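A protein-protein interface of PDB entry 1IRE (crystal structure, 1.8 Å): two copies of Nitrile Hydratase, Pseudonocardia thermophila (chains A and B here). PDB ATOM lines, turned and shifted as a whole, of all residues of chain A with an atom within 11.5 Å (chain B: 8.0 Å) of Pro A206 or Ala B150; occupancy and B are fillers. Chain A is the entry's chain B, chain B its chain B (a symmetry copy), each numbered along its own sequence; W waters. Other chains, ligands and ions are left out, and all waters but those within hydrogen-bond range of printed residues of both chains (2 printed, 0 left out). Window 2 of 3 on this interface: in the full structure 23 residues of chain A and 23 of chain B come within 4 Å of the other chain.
The backbone NH of Ser B151 sits at hydrogen-bond distance from the side-chain carboxylate of Glu A207, 2.8 Å away.
O of Trp A204 lies within hydrogen-bond range of OG of Ser B151, 2.8 Å away.
The side-chain carboxylate (OD2) of Asp A11 is in hydrogen-bond range of the backbone NH (N) of Asn B2 (2.7 Å).
The backbone carbonyl oxygen (O) of Gly A9 lies close to the side-chain amide oxygen (OD1) of Asn B2, 2.9 Å away.
The side-chain hydroxyl of Ser B148 sits at hydrogen-bond distance from the backbone NH of Ala B150.
The side-chain amide nitrogen (ND2) of Asn B2 sits close to the guanidinium group (NH1) of Arg B163.
O of Gly A205 lies close to OE1 of Gln A201 (2.7 Å).
Trp A204 touches Thr B149 (O to O, 3.5 Å).
O of Trp A204 touches C of Ala B150, at 3.96 Å.
Gly A205 touches Thr B149 (N to O, 3.9 Å).
Pro A206 touches Ala B150 (CD to CB, 3.9 Å).
OE1 of Glu A207 touches CA of Ala B150, 3.6 Å away.
Pro B152 touches Glu A207.
Glu A207 touches Lys B153 (O to NZ, 3.8 Å).
Printed residues of chain B within 4 Å of Asp A11: Asn B2.
Of the printed residues of chain B, Trp A204 touches Thr B149, Ala B150 and Ser B151.
Of chain B, only Thr B149 (3.9 Å) comes within 4 Å of Gly A205.
Pro A206 touches just one residue of chain B: Ala B150 (3.9 Å).
Printed residues of chain B within 4 Å of Glu A207: Ala B150 (3.6 Å), Ser B151 (2.8 Å), Pro B152 (3.6 Å) and Lys B153 (3.8 Å).
Of chain A, only Trp A204 and Gly A205 come within 4 Å of Thr B149.
Ala B150 touches just these residues of chain A: Trp A204, Pro A206 and Glu A207.
Printed residues of chain A within 4 Å of Lys B153: Glu A207.
No residue of chain A comes within 4 Å of Arg B158.
The nearest residue of chain B that does not touch Pro A206 is Ser B151 (5.2 Å).
The nearest printed residue of chain A that does not touch Lys B153 is Asp A11 (4.4 Å).
Along chain B the printed residues that touch a printed residue of chain A span positions 2 to 153.
Printed residues of chain A that touch a printed residue of chain B: Gly A9, Asp A11, Trp A204, Gly A205, Pro A206 and Glu A207.
Among the printed residues, 11 pairs touch across the chains.
Among the printed residues, no Asp or Glu carboxylate lies within 4 Å of a Lys or Arg side-chain nitrogen of the other chain.
1 position is printed for both chains.
Water W1 bridges O of Thr B149 (2.6 Å) and O of Leu A203 (3.0 Å).
Water W2 bridges the side-chain amino group of Lys A165 and the backbone carbonyl oxygen of Arg B163.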
ATOM      1  N   GLY A   9      -5.717  15.311  18.340  1.00  0.00           N
ATOM      2  CA  GLY A   9      -5.419  14.639  17.085  1.00  0.00           C
ATOM      3  C   GLY A   9      -3.940  14.439  16.785  1.00  0.00           C
ATOM      4  O   GLY A   9      -3.590  13.749  15.826  1.00  0.00           O
ATOM      5  N   ASP A  11      -0.337  12.919  16.866  1.00  0.00           N
ATOM      6  CA  ASP A  11       0.206  11.573  17.045  1.00  0.00           C
ATOM      7  C   ASP A  11       1.632  11.643  17.602  1.00  0.00           C
ATOM      8  O   ASP A  11       2.300  12.668  17.491  1.00  0.00           O
ATOM      9  CB  ASP A  11       0.267  10.833  15.694  1.00  0.00           C
ATOM     10  CG  ASP A  11      -1.104  10.489  15.132  1.00  0.00           C
ATOM     11  OD1 ASP A  11      -2.015  10.157  15.919  1.00  0.00           O
ATOM     12  OD2 ASP A  11      -1.256  10.504  13.889  1.00  0.00           O
ATOM     13  N   TYR A 161      -8.078  20.421  14.417  1.00  0.00           N
ATOM     14  CA  TYR A 161      -8.775  19.208  13.992  1.00  0.00           C
ATOM     15  C   TYR A 161     -10.243  19.369  13.563  1.00  0.00           C
ATOM     16  O   TYR A 161     -10.777  18.503  12.871  1.00  0.00           O
ATOM     17  CB  TYR A 161      -8.604  18.071  15.018  1.00  0.00           C
ATOM     18  CG  TYR A 161      -9.526  18.092  16.217  1.00  0.00           C
ATOM     19  CD1 TYR A 161      -9.169  18.755  17.392  1.00  0.00           C
ATOM     20  CD2 TYR A 161     -10.737  17.398  16.194  1.00  0.00           C
ATOM     21  CE1 TYR A 161      -9.999  18.722  18.521  1.00  0.00           C
ATOM     22  CE2 TYR A 161     -11.567  17.359  17.305  1.00  0.00           C
ATOM     23  CZ  TYR A 161     -11.197  18.019  18.463  1.00  0.00           C
ATOM     24  OH  TYR A 161     -12.030  17.962  19.554  1.00  0.00           O
ATOM     25  N   ARG A 163     -11.421  22.449  12.098  1.00  0.00           N
ATOM     26  CA  ARG A 163     -11.518  23.462  11.039  1.00  0.00           C
ATOM     27  C   ARG A 163     -11.917  22.899   9.677  1.00  0.00           C
ATOM     28  O   ARG A 163     -11.375  21.887   9.222  1.00  0.00           O
ATOM     29  CB  ARG A 163     -10.212  24.242  10.913  1.00  0.00           C
ATOM     30  CG  ARG A 163      -9.825  24.977  12.182  1.00  0.00           C
ATOM     31  CD  ARG A 163      -8.663  25.913  11.932  1.00  0.00           C
ATOM     32  NE  ARG A 163      -8.040  26.316  13.187  1.00  0.00           N
ATOM     33  CZ  ARG A 163      -6.849  26.896  13.278  1.00  0.00           C
ATOM     34  NH1 ARG A 163      -6.152  27.161  12.181  1.00  0.00           N
ATOM     35  NH2 ARG A 163      -6.318  27.134  14.470  1.00  0.00           N
ATOM     36  N   LYS A 165     -14.472  21.357   8.948  1.00  0.00           N
ATOM     37  CA  LYS A 165     -15.283  20.155   9.090  1.00  0.00           C
ATOM     38  C   LYS A 165     -16.775  20.443   9.236  1.00  0.00           C
ATOM     39  O   LYS A 165     -17.177  21.487   9.751  1.00  0.00           O
ATOM     40  CB  LYS A 165     -14.790  19.311  10.268  1.00  0.00           C
ATOM     41  CG  LYS A 165     -13.343  18.833  10.136  1.00  0.00           C
ATOM     42  CD  LYS A 165     -13.147  17.987   8.883  1.00  0.00           C
ATOM     43  CE  LYS A 165     -11.751  17.369   8.815  1.00  0.00           C
ATOM     44  NZ  LYS A 165     -10.664  18.380   8.709  1.00  0.00           N
ATOM     45  N   THR A 199     -18.697  13.577  13.332  1.00  0.00           N
ATOM     46  CA  THR A 199     -18.423  12.139  13.329  1.00  0.00           C
ATOM     47  C   THR A 199     -16.909  11.936  13.254  1.00  0.00           C
ATOM     48  O   THR A 199     -16.188  12.790  12.733  1.00  0.00           O
ATOM     49  CB  THR A 199     -19.066  11.411  12.125  1.00  0.00           C
ATOM     50  OG1 THR A 199     -18.425  11.828  10.912  1.00  0.00           O
ATOM     51  CG2 THR A 199     -20.558  11.704  12.047  1.00  0.00           C
ATOM     52  N   ALA A 200     -16.434  10.811  13.775  1.00  0.00           N
ATOM     53  CA  ALA A 200     -15.008  10.511  13.751  1.00  0.00           C
ATOM     54  C   ALA A 200     -14.498  10.383  12.312  1.00  0.00           C
ATOM     55  O   ALA A 200     -13.367  10.764  12.017  1.00  0.00           O
ATOM     56  CB  ALA A 200     -14.721   9.242  14.537  1.00  0.00           C
ATOM     57  N   GLN A 201     -15.346   9.876  11.419  1.00  0.00           N
ATOM     58  CA  GLN A 201     -14.977   9.718  10.011  1.00  0.00           C
ATOM     59  C   GLN A 201     -14.801  11.088   9.354  1.00  0.00           C
ATOM     60  O   GLN A 201     -13.946  11.266   8.492  1.00  0.00           O
ATOM     61  CB  GLN A 201     -16.038   8.906   9.255  1.00  0.00           C
ATOM     62  CG  GLN A 201     -16.300   7.502   9.809  1.00  0.00           C
ATOM     63  CD  GLN A 201     -15.156   6.523   9.573  1.00  0.00           C
ATOM     64  OE1 GLN A 201     -13.987   6.845   9.782  1.00  0.00           O
ATOM     65  NE2 GLN A 201     -15.500   5.309   9.154  1.00  0.00           N
ATOM     66  N   GLU A 202     -15.619  12.054   9.764  1.00  0.00           N
ATOM     67  CA  GLU A 202     -15.529  13.410   9.227  1.00  0.00           C
ATOM     68  C   GLU A 202     -14.213  14.059   9.666  1.00  0.00           C
ATOM     69  O   GLU A 202     -13.532  14.713   8.874  1.00  0.00           O
ATOM     70  CB  GLU A 202     -16.720  14.250   9.708  1.00  0.00           C
ATOM     71  CG  GLU A 202     -16.635  15.750   9.395  1.00  0.00           C
ATOM     72  CD  GLU A 202     -16.704  16.082   7.908  1.00  0.00           C
ATOM     73  OE1 GLU A 202     -17.107  15.221   7.096  1.00  0.00           O
ATOM     74  OE2 GLU A 202     -16.352  17.225   7.553  1.00  0.00           O
ATOM     75  N   LEU A 203     -13.843  13.834  10.921  1.00  0.00           N
ATOM     76  CA  LEU A 203     -12.626  14.409  11.476  1.00  0.00           C
ATOM     77  C   LEU A 203     -11.323  13.740  11.042  1.00  0.00           C
ATOM     78  O   LEU A 203     -10.365  14.423  10.679  1.00  0.00           O
ATOM     79  CB  LEU A 203     -12.688  14.395  13.009  1.00  0.00           C
ATOM     80  CG  LEU A 203     -13.807  15.174  13.701  1.00  0.00           C
ATOM     81  CD1 LEU A 203     -13.706  14.965  15.204  1.00  0.00           C
ATOM     82  CD2 LEU A 203     -13.711  16.650  13.361  1.00  0.00           C
ATOM     83  N   TRP A 204     -11.309  12.409  11.049  1.00  0.00           N
ATOM     84  CA  TRP A 204     -10.094  11.653  10.743  1.00  0.00           C
ATOM     85  C   TRP A 204     -10.066  10.869   9.435  1.00  0.00           C
ATOM     86  O   TRP A 204      -9.047  10.258   9.101  1.00  0.00           O
ATOM     87  CB  TRP A 204      -9.799  10.696  11.906  1.00  0.00           C
ATOM     88  CG  TRP A 204     -10.033  11.307  13.263  1.00  0.00           C
ATOM     89  CD1 TRP A 204     -10.956  10.909  14.192  1.00  0.00           C
ATOM     90  CD2 TRP A 204      -9.354  12.437  13.831  1.00  0.00           C
ATOM     91  NE1 TRP A 204     -10.896  11.723  15.300  1.00  0.00           N
ATOM     92  CE2 TRP A 204      -9.922  12.668  15.105  1.00  0.00           C
ATOM     93  CE3 TRP A 204      -8.323  13.278  13.388  1.00  0.00           C
ATOM     94  CZ2 TRP A 204      -9.491  13.705  15.943  1.00  0.00           C
ATOM     95  CZ3 TRP A 204      -7.895  14.313  14.222  1.00  0.00           C
ATOM     96  CH2 TRP A 204      -8.480  14.513  15.486  1.00  0.00           C
ATOM     97  N   GLY A 205     -11.163  10.903   8.685  1.00  0.00           N
ATOM     98  CA  GLY A 205     -11.217  10.159   7.439  1.00  0.00           C
ATOM     99  C   GLY A 205     -11.395   8.681   7.737  1.00  0.00           C
ATOM    100  O   GLY A 205     -11.948   8.326   8.782  1.00  0.00           O
ATOM    101  N   PRO A 206     -10.900   7.789   6.865  1.00  0.00           N
ATOM    102  CA  PRO A 206     -11.035   6.343   7.083  1.00  0.00           C
ATOM    103  C   PRO A 206     -10.415   5.813   8.387  1.00  0.00           C
ATOM    104  O   PRO A 206     -10.850   4.785   8.903  1.00  0.00           O
ATOM    105  CB  PRO A 206     -10.375   5.741   5.838  1.00  0.00           C
ATOM    106  CG  PRO A 206      -9.407   6.805   5.397  1.00  0.00           C
ATOM    107  CD  PRO A 206     -10.193   8.069   5.603  1.00  0.00           C
ATOM    108  N   GLU A 207      -9.431   6.530   8.931  1.00  0.00           N
ATOM    109  CA  GLU A 207      -8.772   6.113  10.175  1.00  0.00           C
ATOM    110  C   GLU A 207      -9.619   6.358  11.425  1.00  0.00           C
ATOM    111  O   GLU A 207      -9.283   5.888  12.513  1.00  0.00           O
ATOM    112  CB  GLU A 207      -7.413   6.801  10.334  1.00  0.00           C
ATOM    113  CG  GLU A 207      -6.327   6.299   9.384  1.00  0.00           C
ATOM    114  CD  GLU A 207      -6.455   6.831   7.959  1.00  0.00           C
ATOM    115  OE1 GLU A 207      -7.220   7.792   7.722  1.00  0.00           O
ATOM    116  OE2 GLU A 207      -5.766   6.289   7.070  1.00  0.00           O
ATOM    117  N   GLY A 208     -10.712   7.097  11.268  1.00  0.00           N
ATOM    118  CA  GLY A 208     -11.577   7.379  12.401  1.00  0.00           C
ATOM    119  C   GLY A 208     -12.412   6.189  12.835  1.00  0.00           C
ATOM    120  O   GLY A 208     -12.722   5.308  12.028  1.00  0.00           O
ATOM    121  N   ASP A 209     -12.760   6.154  14.118  1.00  0.00           N
ATOM    122  CA  ASP A 209     -13.584   5.080  14.678  1.00  0.00           C
ATOM    123  C   ASP A 209     -14.941   5.132  13.961  1.00  0.00           C
ATOM    124  O   ASP A 209     -15.577   6.183  13.895  1.00  0.00           O
ATOM    125  CB  ASP A 209     -13.763   5.297  16.188  1.00  0.00           C
ATOM    126  CG  ASP A 209     -14.365   4.090  16.897  1.00  0.00           C
ATOM    127  OD1 ASP A 209     -15.529   3.743  16.617  1.00  0.00           O
ATOM    128  OD2 ASP A 209     -13.675   3.498  17.750  1.00  0.00           O
ATOM    129  N   PRO A 210     -15.389   3.999  13.398  1.00  0.00           N
ATOM    130  CA  PRO A 210     -16.670   3.945  12.685  1.00  0.00           C
ATOM    131  C   PRO A 210     -17.906   4.179  13.556  1.00  0.00           C
ATOM    132  O   PRO A 210     -19.005   4.373  13.036  1.00  0.00           O
ATOM    133  CB  PRO A 210     -16.660   2.540  12.083  1.00  0.00           C
ATOM    134  CG  PRO A 210     -15.877   1.752  13.088  1.00  0.00           C
ATOM    135  CD  PRO A 210     -14.729   2.682  13.393  1.00  0.00           C
ATOM    136  N   ASN A 211     -17.718   4.196  14.874  1.00  0.00           N
ATOM    137  CA  ASN A 211     -18.828   4.403  15.792  1.00  0.00           C
ATOM    138  C   ASN A 211     -18.449   5.362  16.925  1.00  0.00           C
ATOM    139  O   ASN A 211     -18.553   5.033  18.109  1.00  0.00           O
ATOM    140  CB  ASN A 211     -19.292   3.057  16.356  1.00  0.00           C
ATOM    141  CG  ASN A 211     -20.705   3.107  16.897  1.00  0.00           C
ATOM    142  OD1 ASN A 211     -21.461   4.042  16.626  1.00  0.00           O
ATOM    143  ND2 ASN A 211     -21.074   2.090  17.662  1.00  0.00           N
ATOM    144  N   SER A 212     -18.011   6.555  16.538  1.00  0.00           N
ATOM    145  CA  SER A 212     -17.621   7.575  17.493  1.00  0.00           C
ATOM    146  C   SER A 212     -17.892   8.958  16.919  1.00  0.00           C
ATOM    147  O   SER A 212     -17.895   9.152  15.700  1.00  0.00           O
ATOM    148  CB  SER A 212     -16.134   7.444  17.844  1.00  0.00           C
ATOM    149  OG  SER A 212     -15.742   8.423  18.793  1.00  0.00           O
ATOM    150  N   ASN B   2       0.148  12.348  12.420  1.00  0.00           N
ATOM    151  CA  ASN B   2      -0.102  13.745  12.789  1.00  0.00           C
ATOM    152  C   ASN B   2       0.978  14.173  13.794  1.00  0.00           C
ATOM    153  O   ASN B   2       0.670  14.584  14.913  1.00  0.00           O
ATOM    154  CB  ASN B   2      -1.476  13.899  13.459  1.00  0.00           C
ATOM    155  CG  ASN B   2      -2.640  13.661  12.512  1.00  0.00           C
ATOM    156  OD1 ASN B   2      -3.792  13.570  12.948  1.00  0.00           O
ATOM    157  ND2 ASN B   2      -2.356  13.579  11.223  1.00  0.00           N
ATOM    158  N   PHE B 147      -7.476  17.657  -1.717  1.00  0.00           N
ATOM    159  CA  PHE B 147      -6.553  16.796  -0.974  1.00  0.00           C
ATOM    160  C   PHE B 147      -7.311  15.978   0.072  1.00  0.00           C
ATOM    161  O   PHE B 147      -8.199  16.486   0.759  1.00  0.00           O
ATOM    162  CB  PHE B 147      -5.462  17.641  -0.303  1.00  0.00           C
ATOM    163  CG  PHE B 147      -4.216  16.867   0.056  1.00  0.00           C
ATOM    164  CD1 PHE B 147      -3.083  16.939  -0.752  1.00  0.00           C
ATOM    165  CD2 PHE B 147      -4.163  16.094   1.214  1.00  0.00           C
ATOM    166  CE1 PHE B 147      -1.912  16.254  -0.412  1.00  0.00           C
ATOM    167  CE2 PHE B 147      -2.997  15.402   1.565  1.00  0.00           C
ATOM    168  CZ  PHE B 147      -1.870  15.486   0.750  1.00  0.00           C
ATOM    169  N   SER B 148      -6.944  14.706   0.186  1.00  0.00           N
ATOM    170  CA  SER B 148      -7.564  13.776   1.122  1.00  0.00           C
ATOM    171  C   SER B 148      -7.527  14.232   2.583  1.00  0.00           C
ATOM    172  O   SER B 148      -6.609  14.937   3.002  1.00  0.00           O
ATOM    173  CB  SER B 148      -6.886  12.405   1.001  1.00  0.00           C
ATOM    174  OG  SER B 148      -7.324  11.510   2.007  1.00  0.00           O
ATOM    175  N   THR B 149      -8.552  13.839   3.337  1.00  0.00           N
ATOM    176  CA  THR B 149      -8.636  14.155   4.764  1.00  0.00           C
ATOM    177  C   THR B 149      -8.247  12.924   5.585  1.00  0.00           C
ATOM    178  O   THR B 149      -8.451  12.885   6.802  1.00  0.00           O
ATOM    179  CB  THR B 149     -10.052  14.628   5.176  1.00  0.00           C
ATOM    180  OG1 THR B 149     -11.028  13.653   4.787  1.00  0.00           O
ATOM    181  CG2 THR B 149     -10.375  15.960   4.525  1.00  0.00           C
ATOM    182  N   ALA B 150      -7.687  11.918   4.913  1.00  0.00           N
ATOM    183  CA  ALA B 150      -7.248  10.701   5.583  1.00  0.00           C
ATOM    184  C   ALA B 150      -6.131  11.073   6.549  1.00  0.00           C
ATOM    185  O   ALA B 150      -5.393  12.032   6.316  1.00  0.00           O
ATOM    186  CB  ALA B 150      -6.748   9.677   4.567  1.00  0.00           C
ATOM    187  N   SER B 151      -6.011  10.321   7.634  1.00  0.00           N
ATOM    188  CA  SER B 151      -4.984  10.607   8.627  1.00  0.00           C
ATOM    189  C   SER B 151      -4.276   9.338   9.078  1.00  0.00           C
ATOM    190  O   SER B 151      -4.457   8.880  10.208  1.00  0.00           O
ATOM    191  CB  SER B 151      -5.607  11.328   9.826  1.00  0.00           C
ATOM    192  OG  SER B 151      -6.626  10.543  10.420  1.00  0.00           O
ATOM    193  N   PRO B 152      -3.446   8.757   8.198  1.00  0.00           N
ATOM    194  CA  PRO B 152      -2.715   7.531   8.532  1.00  0.00           C
ATOM    195  C   PRO B 152      -1.824   7.692   9.762  1.00  0.00           C
ATOM    196  O   PRO B 152      -1.208   8.737   9.967  1.00  0.00           O
ATOM    197  CB  PRO B 152      -1.904   7.259   7.261  1.00  0.00           C
ATOM    198  CG  PRO B 152      -1.701   8.623   6.678  1.00  0.00           C
ATOM    199  CD  PRO B 152      -3.059   9.253   6.866  1.00  0.00           C
ATOM    200  N   LYS B 153      -1.801   6.662  10.600  1.00  0.00           N
ATOM    201  CA  LYS B 153      -0.993   6.679  11.807  1.00  0.00           C
ATOM    202  C   LYS B 153       0.471   6.361  11.495  1.00  0.00           C
ATOM    203  O   LYS B 153       1.365   6.636  12.300  1.00  0.00           O
ATOM    204  CB  LYS B 153      -1.597   5.727  12.840  1.00  0.00           C
ATOM    205  CG  LYS B 153      -2.931   6.260  13.352  1.00  0.00           C
ATOM    206  CD  LYS B 153      -3.898   5.182  13.788  1.00  0.00           C
ATOM    207  CE  LYS B 153      -5.274   5.799  14.048  1.00  0.00           C
ATOM    208  NZ  LYS B 153      -6.285   4.800  14.502  1.00  0.00           N
ATOM    209  N   ALA B 156       3.472   9.115   5.948  1.00  0.00           N
ATOM    210  CA  ALA B 156       2.778   9.689   4.802  1.00  0.00           C
ATOM    211  C   ALA B 156       3.317  11.105   4.613  1.00  0.00           C
ATOM    212  O   ALA B 156       3.975  11.645   5.505  1.00  0.00           O
ATOM    213  CB  ALA B 156       1.271   9.719   5.039  1.00  0.00           C
ATOM    214  N   ARG B 158       1.433  13.866   3.992  1.00  0.00           N
ATOM    215  CA  ARG B 158       0.163  14.581   3.988  1.00  0.00           C
ATOM    216  C   ARG B 158       0.175  15.679   5.045  1.00  0.00           C
ATOM    217  O   ARG B 158      -0.439  15.528   6.102  1.00  0.00           O
ATOM    218  CB  ARG B 158      -0.974  13.600   4.292  1.00  0.00           C
ATOM    219  CG  ARG B 158      -1.032  12.397   3.362  1.00  0.00           C
ATOM    220  CD  ARG B 158      -1.905  11.300   3.950  1.00  0.00           C
ATOM    221  NE  ARG B 158      -2.004  10.141   3.067  1.00  0.00           N
ATOM    222  CZ  ARG B 158      -3.044   9.874   2.282  1.00  0.00           C
ATOM    223  NH1 ARG B 158      -4.099  10.683   2.260  1.00  0.00           N
ATOM    224  NH2 ARG B 158      -3.032   8.787   1.519  1.00  0.00           N
ATOM    225  N   ALA B 159       0.857  16.786   4.755  1.00  0.00           N
ATOM    226  CA  ALA B 159       0.933  17.900   5.707  1.00  0.00           C
ATOM    227  C   ALA B 159      -0.469  18.312   6.139  1.00  0.00           C
ATOM    228  O   ALA B 159      -1.363  18.473   5.308  1.00  0.00           O
ATOM    229  CB  ALA B 159       1.663  19.079   5.091  1.00  0.00           C
ATOM    230  N   ARG B 160      -0.667  18.450   7.445  1.00  0.00           N
ATOM    231  CA  ARG B 160      -1.973  18.821   7.961  1.00  0.00           C
ATOM    232  C   ARG B 160      -2.543  20.084   7.322  1.00  0.00           C
ATOM    233  O   ARG B 160      -3.746  20.151   7.061  1.00  0.00           O
ATOM    234  CB  ARG B 160      -1.929  18.969   9.485  1.00  0.00           C
ATOM    235  CG  ARG B 160      -1.890  17.637  10.236  1.00  0.00           C
ATOM    236  CD  ARG B 160      -1.634  17.850  11.731  1.00  0.00           C
ATOM    237  NE  ARG B 160      -0.328  18.470  11.959  1.00  0.00           N
ATOM    238  CZ  ARG B 160       0.148  18.827  13.149  1.00  0.00           C
ATOM    239  NH1 ARG B 160      -0.569  18.633  14.250  1.00  0.00           N
ATOM    240  NH2 ARG B 160       1.353  19.377  13.235  1.00  0.00           N
ATOM    241  N   ARG B 163      -4.559  19.228   3.969  1.00  0.00           N
ATOM    242  CA  ARG B 163      -5.660  18.258   4.000  1.00  0.00           C
ATOM    243  C   ARG B 163      -7.043  18.882   3.834  1.00  0.00           C
ATOM    244  O   ARG B 163      -7.370  19.886   4.472  1.00  0.00           O
ATOM    245  CB  ARG B 163      -5.618  17.430   5.283  1.00  0.00           C
ATOM    246  CG  ARG B 163      -4.335  16.638   5.446  1.00  0.00           C
ATOM    247  CD  ARG B 163      -4.443  15.665   6.600  1.00  0.00           C
ATOM    248  NE  ARG B 163      -3.125  15.196   7.010  1.00  0.00           N
ATOM    249  CZ  ARG B 163      -2.878  14.567   8.153  1.00  0.00           C
ATOM    250  NH1 ARG B 163      -3.866  14.310   9.000  1.00  0.00           N
ATOM    251  NH2 ARG B 163      -1.629  14.267   8.487  1.00  0.00           N
ATOM    252  N   GLY B 164      -7.838  18.279   2.955  1.00  0.00           N
ATOM    253  CA  GLY B 164      -9.183  18.759   2.693  1.00  0.00           C
ATOM    254  C   GLY B 164      -9.248  20.030   1.871  1.00  0.00           C
ATOM    255  O   GLY B 164     -10.339  20.527   1.586  1.00  0.00           O
ATOM    256  N   ASP B 180       3.406   6.298   1.575  1.00  0.00           N
ATOM    257  CA  ASP B 180       2.475   5.579   2.451  1.00  0.00           C
ATOM    258  C   ASP B 180       2.745   4.085   2.549  1.00  0.00           C
ATOM    259  O   ASP B 180       2.376   3.448   3.536  1.00  0.00           O
ATOM    260  CB  ASP B 180       1.019   5.873   2.066  1.00  0.00           C
ATOM    261  CG  ASP B 180       0.684   7.362   2.137  1.00  0.00           C
ATOM    262  OD1 ASP B 180      -0.444   7.714   2.533  1.00  0.00           O
ATOM    263  OD2 ASP B 180       1.554   8.185   1.792  1.00  0.00           O
ATOM    264  N   PRO B 221      -3.142   8.953  -4.979  1.00  0.00           N
ATOM    265  CA  PRO B 221      -4.187   8.633  -3.994  1.00  0.00           C
ATOM    266  C   PRO B 221      -4.543   9.795  -3.053  1.00  0.00           C
ATOM    267  O   PRO B 221      -5.609   9.794  -2.426  1.00  0.00           O
ATOM    268  CB  PRO B 221      -3.572   7.469  -3.210  1.00  0.00           C
ATOM    269  CG  PRO B 221      -2.597   6.862  -4.174  1.00  0.00           C
ATOM    270  CD  PRO B 221      -1.972   8.078  -4.795  1.00  0.00           C
ATOM    271  N   TYR B 222      -3.661  10.790  -2.982  1.00  0.00           N
ATOM    272  CA  TYR B 222      -3.857  11.959  -2.118  1.00  0.00           C
ATOM    273  C   TYR B 222      -4.935  12.919  -2.592  1.00  0.00           C
ATOM    274  O   TYR B 222      -5.448  13.713  -1.805  1.00  0.00           O
ATOM    275  CB  TYR B 222      -2.567  12.780  -2.026  1.00  0.00           C
ATOM    276  CG  TYR B 222      -1.434  12.190  -1.219  1.00  0.00           C
ATOM    277  CD1 TYR B 222      -1.465  10.872  -0.769  1.00  0.00           C
ATOM    278  CD2 TYR B 222      -0.325  12.972  -0.898  1.00  0.00           C
ATOM    279  CE1 TYR B 222      -0.412  10.350  -0.015  1.00  0.00           C
ATOM    280  CE2 TYR B 222       0.725  12.465  -0.150  1.00  0.00           C
ATOM    281  CZ  TYR B 222       0.675  11.155   0.291  1.00  0.00           C
ATOM    282  OH  TYR B 222       1.711  10.670   1.053  1.00  0.00           O
HETATM  283  O   HOH W   1      -7.890  14.116   9.040  1.00  0.00           O
HETATM  284  O   HOH W   2      -7.896  19.330   7.854  1.00  0.00           O
